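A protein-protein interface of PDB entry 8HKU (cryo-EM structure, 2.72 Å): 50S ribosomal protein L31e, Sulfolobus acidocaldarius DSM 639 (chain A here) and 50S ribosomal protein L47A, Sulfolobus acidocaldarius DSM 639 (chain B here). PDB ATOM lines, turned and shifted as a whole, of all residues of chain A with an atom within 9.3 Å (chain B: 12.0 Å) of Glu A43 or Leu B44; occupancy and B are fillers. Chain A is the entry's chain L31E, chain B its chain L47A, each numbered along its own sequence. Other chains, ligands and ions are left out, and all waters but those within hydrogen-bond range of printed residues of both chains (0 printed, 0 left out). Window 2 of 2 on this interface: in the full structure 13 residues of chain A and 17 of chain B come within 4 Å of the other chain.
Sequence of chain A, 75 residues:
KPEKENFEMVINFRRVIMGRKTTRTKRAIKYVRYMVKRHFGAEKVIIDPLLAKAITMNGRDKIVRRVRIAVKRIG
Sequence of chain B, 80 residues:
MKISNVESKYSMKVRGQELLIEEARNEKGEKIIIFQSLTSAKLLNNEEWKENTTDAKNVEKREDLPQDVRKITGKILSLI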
ATOM      1  N   PRO A   2     -15.518 -26.975  26.119  1.00  0.00           N
ATOM      2  CA  PRO A   2     -16.313 -25.983  26.853  1.00  0.00           C
ATOM      3  C   PRO A   2     -17.715 -25.864  26.277  1.00  0.00           C
ATOM      4  O   PRO A   2     -17.910 -25.878  25.060  1.00  0.00           O
ATOM      5  CB  PRO A   2     -15.515 -24.686  26.676  1.00  0.00           C
ATOM      6  CG  PRO A   2     -14.702 -24.910  25.441  1.00  0.00           C
ATOM      7  CD  PRO A   2     -14.359 -26.368  25.445  1.00  0.00           C
ATOM      8  N   LYS A   4     -21.120 -24.437  24.980  1.00  0.00           N
ATOM      9  CA  LYS A   4     -21.619 -23.249  24.285  1.00  0.00           C
ATOM     10  C   LYS A   4     -22.854 -22.746  25.027  1.00  0.00           C
ATOM     11  O   LYS A   4     -24.000 -22.934  24.610  1.00  0.00           O
ATOM     12  CB  LYS A   4     -21.928 -23.564  22.826  1.00  0.00           C
ATOM     13  CG  LYS A   4     -20.728 -24.028  22.019  1.00  0.00           C
ATOM     14  CD  LYS A   4     -19.801 -22.867  21.688  1.00  0.00           C
ATOM     15  CE  LYS A   4     -18.515 -22.961  22.479  1.00  0.00           C
ATOM     16  NZ  LYS A   4     -17.556 -21.907  22.080  1.00  0.00           N
ATOM     17  N   ARG A  33     -13.909  -7.831  29.559  1.00  0.00           N
ATOM     18  CA  ARG A  33     -13.195  -8.804  28.740  1.00  0.00           C
ATOM     19  C   ARG A  33     -12.518  -9.853  29.599  1.00  0.00           C
ATOM     20  O   ARG A  33     -12.491 -11.033  29.243  1.00  0.00           O
ATOM     21  CB  ARG A  33     -12.161  -8.110  27.867  1.00  0.00           C
ATOM     22  CG  ARG A  33     -12.744  -7.365  26.720  1.00  0.00           C
ATOM     23  CD  ARG A  33     -11.667  -6.857  25.805  1.00  0.00           C
ATOM     24  NE  ARG A  33     -12.201  -6.524  24.492  1.00  0.00           N
ATOM     25  CZ  ARG A  33     -12.507  -5.298  24.097  1.00  0.00           C
ATOM     26  NH1 ARG A  33     -12.354  -4.257  24.892  1.00  0.00           N
ATOM     27  NH2 ARG A  33     -12.986  -5.115  22.874  1.00  0.00           N
ATOM     28  N   VAL A  36     -15.243 -12.316  31.088  1.00  0.00           N
ATOM     29  CA  VAL A  36     -15.796 -13.272  30.138  1.00  0.00           C
ATOM     30  C   VAL A  36     -14.779 -14.361  29.830  1.00  0.00           C
ATOM     31  O   VAL A  36     -15.136 -15.529  29.670  1.00  0.00           O
ATOM     32  CB  VAL A  36     -16.284 -12.554  28.868  1.00  0.00           C
ATOM     33  CG1 VAL A  36     -16.690 -13.555  27.815  1.00  0.00           C
ATOM     34  CG2 VAL A  36     -17.451 -11.666  29.197  1.00  0.00           C
ATOM     35  N   LYS A  37     -13.499 -14.008  29.759  1.00  0.00           N
ATOM     36  CA  LYS A  37     -12.475 -15.024  29.568  1.00  0.00           C
ATOM     37  C   LYS A  37     -12.292 -15.908  30.793  1.00  0.00           C
ATOM     38  O   LYS A  37     -11.903 -17.069  30.651  1.00  0.00           O
ATOM     39  CB  LYS A  37     -11.144 -14.376  29.219  1.00  0.00           C
ATOM     40  CG  LYS A  37     -11.138 -13.615  27.926  1.00  0.00           C
ATOM     41  CD  LYS A  37      -9.795 -12.966  27.717  1.00  0.00           C
ATOM     42  CE  LYS A  37      -9.803 -12.045  26.530  1.00  0.00           C
ATOM     43  NZ  LYS A  37      -8.584 -11.200  26.528  1.00  0.00           N
ATOM     44  N   ARG A  38     -12.533 -15.384  31.991  1.00  0.00           N
ATOM     45  CA  ARG A  38     -12.348 -16.182  33.194  1.00  0.00           C
ATOM     46  C   ARG A  38     -13.464 -17.198  33.372  1.00  0.00           C
ATOM     47  O   ARG A  38     -13.205 -18.351  33.725  1.00  0.00           O
ATOM     48  CB  ARG A  38     -12.257 -15.273  34.417  1.00  0.00           C
ATOM     49  CG  ARG A  38     -12.243 -16.013  35.728  1.00  0.00           C
ATOM     50  CD  ARG A  38     -12.179 -15.055  36.883  1.00  0.00           C
ATOM     51  NE  ARG A  38     -12.316 -15.726  38.164  1.00  0.00           N
ATOM     52  CZ  ARG A  38     -12.664 -15.119  39.286  1.00  0.00           C
ATOM     53  NH1 ARG A  38     -12.912 -13.824  39.319  1.00  0.00           N
ATOM     54  NH2 ARG A  38     -12.771 -15.830  40.400  1.00  0.00           N
ATOM     55  N   PHE A  40     -15.746 -18.225  30.998  1.00  0.00           N
ATOM     56  CA  PHE A  40     -16.211 -18.909  29.799  1.00  0.00           C
ATOM     57  C   PHE A  40     -15.103 -19.480  28.932  1.00  0.00           C
ATOM     58  O   PHE A  40     -15.408 -20.125  27.926  1.00  0.00           O
ATOM     59  CB  PHE A  40     -17.066 -17.975  28.932  1.00  0.00           C
ATOM     60  CG  PHE A  40     -18.308 -17.501  29.601  1.00  0.00           C
ATOM     61  CD1 PHE A  40     -19.447 -18.269  29.592  1.00  0.00           C
ATOM     62  CD2 PHE A  40     -18.341 -16.283  30.232  1.00  0.00           C
ATOM     63  CE1 PHE A  40     -20.579 -17.834  30.211  1.00  0.00           C
ATOM     64  CE2 PHE A  40     -19.472 -15.845  30.851  1.00  0.00           C
ATOM     65  CZ  PHE A  40     -20.594 -16.622  30.839  1.00  0.00           C
ATOM     66  N   GLY A  41     -13.841 -19.262  29.271  1.00  0.00           N
ATOM     67  CA  GLY A  41     -12.775 -19.759  28.431  1.00  0.00           C
ATOM     68  C   GLY A  41     -12.673 -19.094  27.084  1.00  0.00           C
ATOM     69  O   GLY A  41     -12.053 -19.651  26.179  1.00  0.00           O
ATOM     70  N   ALA A  42     -13.263 -17.914  26.921  1.00  0.00           N
ATOM     71  CA  ALA A  42     -13.196 -17.211  25.650  1.00  0.00           C
ATOM     72  C   ALA A  42     -11.772 -16.764  25.362  1.00  0.00           C
ATOM     73  O   ALA A  42     -11.055 -16.315  26.255  1.00  0.00           O
ATOM     74  CB  ALA A  42     -14.125 -16.002  25.664  1.00  0.00           C
ATOM     75  N   GLU A  43     -11.359 -16.898  24.108  1.00  0.00           N
ATOM     76  CA  GLU A  43     -10.080 -16.357  23.673  1.00  0.00           C
ATOM     77  C   GLU A  43     -10.214 -15.015  22.974  1.00  0.00           C
ATOM     78  O   GLU A  43      -9.248 -14.250  22.938  1.00  0.00           O
ATOM     79  CB  GLU A  43      -9.368 -17.346  22.753  1.00  0.00           C
ATOM     80  CG  GLU A  43      -8.937 -18.609  23.463  1.00  0.00           C
ATOM     81  CD  GLU A  43      -8.252 -19.595  22.543  1.00  0.00           C
ATOM     82  OE1 GLU A  43      -8.224 -19.350  21.319  1.00  0.00           O
ATOM     83  OE2 GLU A  43      -7.745 -20.620  23.044  1.00  0.00           O
ATOM     84  N   LYS A  44     -11.385 -14.716  22.418  1.00  0.00           N
ATOM     85  CA  LYS A  44     -11.691 -13.399  21.882  1.00  0.00           C
ATOM     86  C   LYS A  44     -13.071 -12.991  22.366  1.00  0.00           C
ATOM     87  O   LYS A  44     -14.009 -13.790  22.315  1.00  0.00           O
ATOM     88  CB  LYS A  44     -11.632 -13.391  20.357  1.00  0.00           C
ATOM     89  CG  LYS A  44     -12.135 -12.107  19.739  1.00  0.00           C
ATOM     90  CD  LYS A  44     -11.964 -12.112  18.239  1.00  0.00           C
ATOM     91  CE  LYS A  44     -12.702 -10.950  17.610  1.00  0.00           C
ATOM     92  NZ  LYS A  44     -12.297 -10.741  16.195  1.00  0.00           N
ATOM     93  N   VAL A  45     -13.196 -11.755  22.833  1.00  0.00           N
ATOM     94  CA  VAL A  45     -14.442 -11.240  23.379  1.00  0.00           C
ATOM     95  C   VAL A  45     -14.878 -10.045  22.549  1.00  0.00           C
ATOM     96  O   VAL A  45     -14.067  -9.167  22.244  1.00  0.00           O
ATOM     97  CB  VAL A  45     -14.294 -10.849  24.858  1.00  0.00           C
ATOM     98  CG1 VAL A  45     -15.600 -10.333  25.394  1.00  0.00           C
ATOM     99  CG2 VAL A  45     -13.825 -12.031  25.660  1.00  0.00           C
ATOM    100  N   ILE A  46     -16.154 -10.015  22.187  1.00  0.00           N
ATOM    101  CA  ILE A  46     -16.751  -8.907  21.457  1.00  0.00           C
ATOM    102  C   ILE A  46     -17.779  -8.251  22.363  1.00  0.00           C
ATOM    103  O   ILE A  46     -18.658  -8.930  22.901  1.00  0.00           O
ATOM    104  CB  ILE A  46     -17.388  -9.384  20.144  1.00  0.00           C
ATOM    105  CG1 ILE A  46     -16.314  -9.958  19.227  1.00  0.00           C
ATOM    106  CG2 ILE A  46     -18.123  -8.260  19.471  1.00  0.00           C
ATOM    107  CD1 ILE A  46     -16.795 -10.280  17.859  1.00  0.00           C
ATOM    108  N   ARG A  73     -22.071 -17.122  23.916  1.00  0.00           N
ATOM    109  CA  ARG A  73     -20.677 -17.462  23.666  1.00  0.00           C
ATOM    110  C   ARG A  73     -20.675 -18.567  22.616  1.00  0.00           C
ATOM    111  O   ARG A  73     -20.633 -19.761  22.913  1.00  0.00           O
ATOM    112  CB  ARG A  73     -19.955 -17.852  24.956  1.00  0.00           C
ATOM    113  CG  ARG A  73     -18.471 -18.177  24.798  1.00  0.00           C
ATOM    114  CD  ARG A  73     -17.772 -16.852  24.478  1.00  0.00           C
ATOM    115  NE  ARG A  73     -17.786 -16.575  23.046  1.00  0.00           N
ATOM    116  CZ  ARG A  73     -17.445 -15.430  22.471  1.00  0.00           C
ATOM    117  NH1 ARG A  73     -17.283 -14.324  23.172  1.00  0.00           N
ATOM    118  NH2 ARG A  73     -17.310 -15.389  21.150  1.00  0.00           N
ATOM    119  N   ILE A  74     -20.721 -18.143  21.361  1.00  0.00           N
ATOM    120  CA  ILE A  74     -20.707 -19.044  20.221  1.00  0.00           C
ATOM    121  C   ILE A  74     -19.316 -19.651  20.078  1.00  0.00           C
ATOM    122  O   ILE A  74     -18.377 -19.246  20.771  1.00  0.00           O
ATOM    123  CB  ILE A  74     -21.135 -18.303  18.946  1.00  0.00           C
ATOM    124  CG1 ILE A  74     -20.215 -17.118  18.690  1.00  0.00           C
ATOM    125  CG2 ILE A  74     -22.552 -17.806  19.086  1.00  0.00           C
ATOM    126  CD1 ILE A  74     -19.446 -17.246  17.426  1.00  0.00           C
ATOM    127  N   GLY A  75     -19.186 -20.655  19.214  1.00  0.00           N
ATOM    128  CA  GLY A  75     -17.904 -21.291  18.952  1.00  0.00           C
ATOM    129  C   GLY A  75     -16.937 -20.477  18.113  1.00  0.00           C
ATOM    130  O   GLY A  75     -17.336 -19.583  17.371  1.00  0.00           O
ATOM    131  OXT GLY A  75     -15.729 -20.704  18.156  1.00  0.00           O
ATOM    132  N   SER B  40     -23.274  -8.541  12.522  1.00  0.00           N
ATOM    133  CA  SER B  40     -22.135  -9.224  11.936  1.00  0.00           C
ATOM    134  C   SER B  40     -20.864  -8.820  12.663  1.00  0.00           C
ATOM    135  O   SER B  40     -20.720  -7.677  13.106  1.00  0.00           O
ATOM    136  CB  SER B  40     -22.014  -8.907  10.443  1.00  0.00           C
ATOM    137  OG  SER B  40     -21.899  -7.513  10.225  1.00  0.00           O
ATOM    138  N   ALA B  41     -19.940  -9.769  12.780  1.00  0.00           N
ATOM    139  CA  ALA B  41     -18.656  -9.509  13.416  1.00  0.00           C
ATOM    140  C   ALA B  41     -17.666 -10.577  12.981  1.00  0.00           C
ATOM    141  O   ALA B  41     -18.041 -11.621  12.445  1.00  0.00           O
ATOM    142  CB  ALA B  41     -18.782  -9.469  14.941  1.00  0.00           C
ATOM    143  N   LYS B  42     -16.391 -10.298  13.222  1.00  0.00           N
ATOM    144  CA  LYS B  42     -15.329 -11.244  12.933  1.00  0.00           C
ATOM    145  C   LYS B  42     -15.341 -12.384  13.947  1.00  0.00           C
ATOM    146  O   LYS B  42     -15.984 -12.316  14.996  1.00  0.00           O
ATOM    147  CB  LYS B  42     -13.973 -10.544  12.952  1.00  0.00           C
ATOM    148  CG  LYS B  42     -13.702  -9.677  11.748  1.00  0.00           C
ATOM    149  CD  LYS B  42     -13.132 -10.483  10.604  1.00  0.00           C
ATOM    150  CE  LYS B  42     -11.716 -10.916  10.919  1.00  0.00           C
ATOM    151  NZ  LYS B  42     -10.837  -9.753  11.216  1.00  0.00           N
ATOM    152  N   LEU B  43     -14.621 -13.446  13.619  1.00  0.00           N
ATOM    153  CA  LEU B  43     -14.401 -14.564  14.521  1.00  0.00           C
ATOM    154  C   LEU B  43     -12.918 -14.639  14.857  1.00  0.00           C
ATOM    155  O   LEU B  43     -12.108 -13.860  14.353  1.00  0.00           O
ATOM    156  CB  LEU B  43     -14.900 -15.875  13.909  1.00  0.00           C
ATOM    157  CG  LEU B  43     -16.415 -16.068  13.928  1.00  0.00           C
ATOM    158  CD1 LEU B  43     -16.786 -17.486  13.547  1.00  0.00           C
ATOM    159  CD2 LEU B  43     -16.965 -15.720  15.292  1.00  0.00           C
ATOM    160  N   LEU B  44     -12.565 -15.590  15.721  1.00  0.00           N
ATOM    161  CA  LEU B  44     -11.181 -15.710  16.165  1.00  0.00           C
ATOM    162  C   LEU B  44     -10.254 -15.999  14.993  1.00  0.00           C
ATOM    163  O   LEU B  44      -9.349 -15.214  14.691  1.00  0.00           O
ATOM    164  CB  LEU B  44     -11.067 -16.798  17.233  1.00  0.00           C
ATOM    165  CG  LEU B  44      -9.651 -17.210  17.633  1.00  0.00           C
ATOM    166  CD1 LEU B  44      -9.011 -16.158  18.516  1.00  0.00           C
ATOM    167  CD2 LEU B  44      -9.684 -18.547  18.343  1.00  0.00           C
ATOM    168  N   ASN B  45     -10.472 -17.120  14.310  1.00  0.00           N
ATOM    169  CA  ASN B  45      -9.621 -17.509  13.189  1.00  0.00           C
ATOM    170  C   ASN B  45     -10.419 -18.411  12.258  1.00  0.00           C
ATOM    171  O   ASN B  45     -10.680 -19.566  12.605  1.00  0.00           O
ATOM    172  CB  ASN B  45      -8.359 -18.222  13.675  1.00  0.00           C
ATOM    173  CG  ASN B  45      -7.298 -17.263  14.175  1.00  0.00           C
ATOM    174  OD1 ASN B  45      -6.903 -17.307  15.339  1.00  0.00           O
ATOM    175  ND2 ASN B  45      -6.827 -16.390  13.293  1.00  0.00           N
ATOM    176  N   ASN B  46     -10.815 -17.904  11.091  1.00  0.00           N
ATOM    177  CA  ASN B  46     -10.812 -16.484  10.738  1.00  0.00           C
ATOM    178  C   ASN B  46     -11.891 -16.281   9.687  1.00  0.00           C
ATOM    179  O   ASN B  46     -11.638 -16.473   8.499  1.00  0.00           O
ATOM    180  CB  ASN B  46      -9.458 -16.023  10.189  1.00  0.00           C
ATOM    181  CG  ASN B  46      -9.345 -14.512  10.115  1.00  0.00           C
ATOM    182  OD1 ASN B  46     -10.279 -13.791  10.461  1.00  0.00           O
ATOM    183  ND2 ASN B  46      -8.198 -14.026   9.661  1.00  0.00           N
ATOM    184  N   GLU B  47     -13.088 -15.889  10.102  1.00  0.00           N
ATOM    185  CA  GLU B  47     -14.204 -15.829   9.169  1.00  0.00           C
ATOM    186  C   GLU B  47     -15.241 -14.854   9.708  1.00  0.00           C
ATOM    187  O   GLU B  47     -14.981 -14.101  10.653  1.00  0.00           O
ATOM    188  CB  GLU B  47     -14.784 -17.227   8.925  1.00  0.00           C
ATOM    189  CG  GLU B  47     -15.394 -17.885  10.149  1.00  0.00           C
ATOM    190  CD  GLU B  47     -14.483 -18.937  10.762  1.00  0.00           C
ATOM    191  OE1 GLU B  47     -13.281 -18.959  10.425  1.00  0.00           O
ATOM    192  OE2 GLU B  47     -14.971 -19.746  11.580  1.00  0.00           O
ATOM    193  N   GLU B  48     -16.419 -14.867   9.098  1.00  0.00           N
ATOM    194  CA  GLU B  48     -17.469 -13.898   9.362  1.00  0.00           C
ATOM    195  C   GLU B  48     -18.664 -14.602   9.991  1.00  0.00           C
ATOM    196  O   GLU B  48     -19.050 -15.690   9.558  1.00  0.00           O
ATOM    197  CB  GLU B  48     -17.887 -13.205   8.061  1.00  0.00           C
ATOM    198  CG  GLU B  48     -18.948 -12.129   8.201  1.00  0.00           C
ATOM    199  CD  GLU B  48     -18.477 -10.936   9.003  1.00  0.00           C
ATOM    200  OE1 GLU B  48     -17.254 -10.684   9.042  1.00  0.00           O
ATOM    201  OE2 GLU B  48     -19.331 -10.244   9.589  1.00  0.00           O
ATOM    202  N   TRP B  49     -19.242 -13.982  11.013  1.00  0.00           N
ATOM    203  CA  TRP B  49     -20.434 -14.501  11.666  1.00  0.00           C
ATOM    204  C   TRP B  49     -21.593 -13.544  11.429  1.00  0.00           C
ATOM    205  O   TRP B  49     -21.419 -12.324  11.483  1.00  0.00           O
ATOM    206  CB  TRP B  49     -20.210 -14.691  13.170  1.00  0.00           C
ATOM    207  CG  TRP B  49     -21.472 -14.952  13.927  1.00  0.00           C
ATOM    208  CD1 TRP B  49     -22.110 -16.146  14.060  1.00  0.00           C
ATOM    209  CD2 TRP B  49     -22.252 -13.998  14.655  1.00  0.00           C
ATOM    210  NE1 TRP B  49     -23.241 -15.998  14.823  1.00  0.00           N
ATOM    211  CE2 TRP B  49     -23.351 -14.687  15.201  1.00  0.00           C
ATOM    212  CE3 TRP B  49     -22.128 -12.627  14.898  1.00  0.00           C
ATOM    213  CZ2 TRP B  49     -24.317 -14.055  15.973  1.00  0.00           C
ATOM    214  CZ3 TRP B  49     -23.090 -12.002  15.665  1.00  0.00           C
ATOM    215  CH2 TRP B  49     -24.170 -12.714  16.193  1.00  0.00           C
ATOM    216  N   LYS B  50     -22.771 -14.097  11.159  1.00  0.00           N
ATOM    217  CA  LYS B  50     -23.958 -13.297  10.899  1.00  0.00           C
ATOM    218  C   LYS B  50     -25.103 -13.777  11.776  1.00  0.00           C
ATOM    219  O   LYS B  50     -25.430 -14.967  11.780  1.00  0.00           O
ATOM    220  CB  LYS B  50     -24.358 -13.367   9.424  1.00  0.00           C
ATOM    221  CG  LYS B  50     -25.552 -12.504   9.075  1.00  0.00           C
ATOM    222  CD  LYS B  50     -25.219 -11.030   9.225  1.00  0.00           C
ATOM    223  CE  LYS B  50     -24.263 -10.557   8.142  1.00  0.00           C
ATOM    224  NZ  LYS B  50     -24.924 -10.481   6.812  1.00  0.00           N
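Hydrophobic or aromatic side chains of chain B within 4 Å of the printed part of chain A: Ala B41, Leu B43 and Leu B44. Hydrophobic or aromatic side chains of chain A within 4 Å of the printed part of chain B: Ile A46 and Ile A74. Among the printed residues, 6 pairs touch across the chains. Among the printed residues, no Asp or Glu carboxylate lies within 4 Å of a Lys or Arg side-chain nitrogen of the other chain.
Leu B44 touches Glu A43 (CD2 to OE1, 3.4 Å). Lys B42 touches Lys A44 (CB to NZ, 3.7 Å). Leu B43 touches Lys A44. Ala B41 touches Ile A46. Ile A46 touches Lys B42. CD2 of Leu B43 touches CD1 of Ile A74 (3.6 Å).
The side-chain amino group (NZ) of Lys A4 sits at hydrogen-bond distance from the backbone carbonyl oxygen (O) of Ile A74 (3.1 Å). The guanidinium group (NH1) of Arg A73 sits at hydrogen-bond distance from the backbone carbonyl oxygen (O) of Lys A44 (3.4 Å). The backbone NH (N) of Ala B41 is in hydrogen-bond range of the side-chain carboxylate (OE2) of Glu B48 (3.3 Å). N of Trp B49 lies within hydrogen-bond range of O of Ala B41 (3.0 Å).
Of chain B, only Leu B44 comes within 4 Å of Glu A43. Leu B44 touches one residue of chain A. Lys A37 touches none of the printed residues of chain B. No residue of chain B comes within 4 Å of Ala A42. Lys A44 touches just these residues of chain B: Lys B42 (3.7 Å) and Leu B43 (3.6 Å). No residue of chain B comes within 4 Å of Val A45. Printed residues of chain B within 4 Å of Ile A46: Ala B41 and Lys B42. Of the printed residues of chain B, Ile A74 touches Leu B43. Val A36 touches none of the printed residues of chain B. The nearest residue of chain B that does not touch Glu A43 is Asn B45 (6.5 Å).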
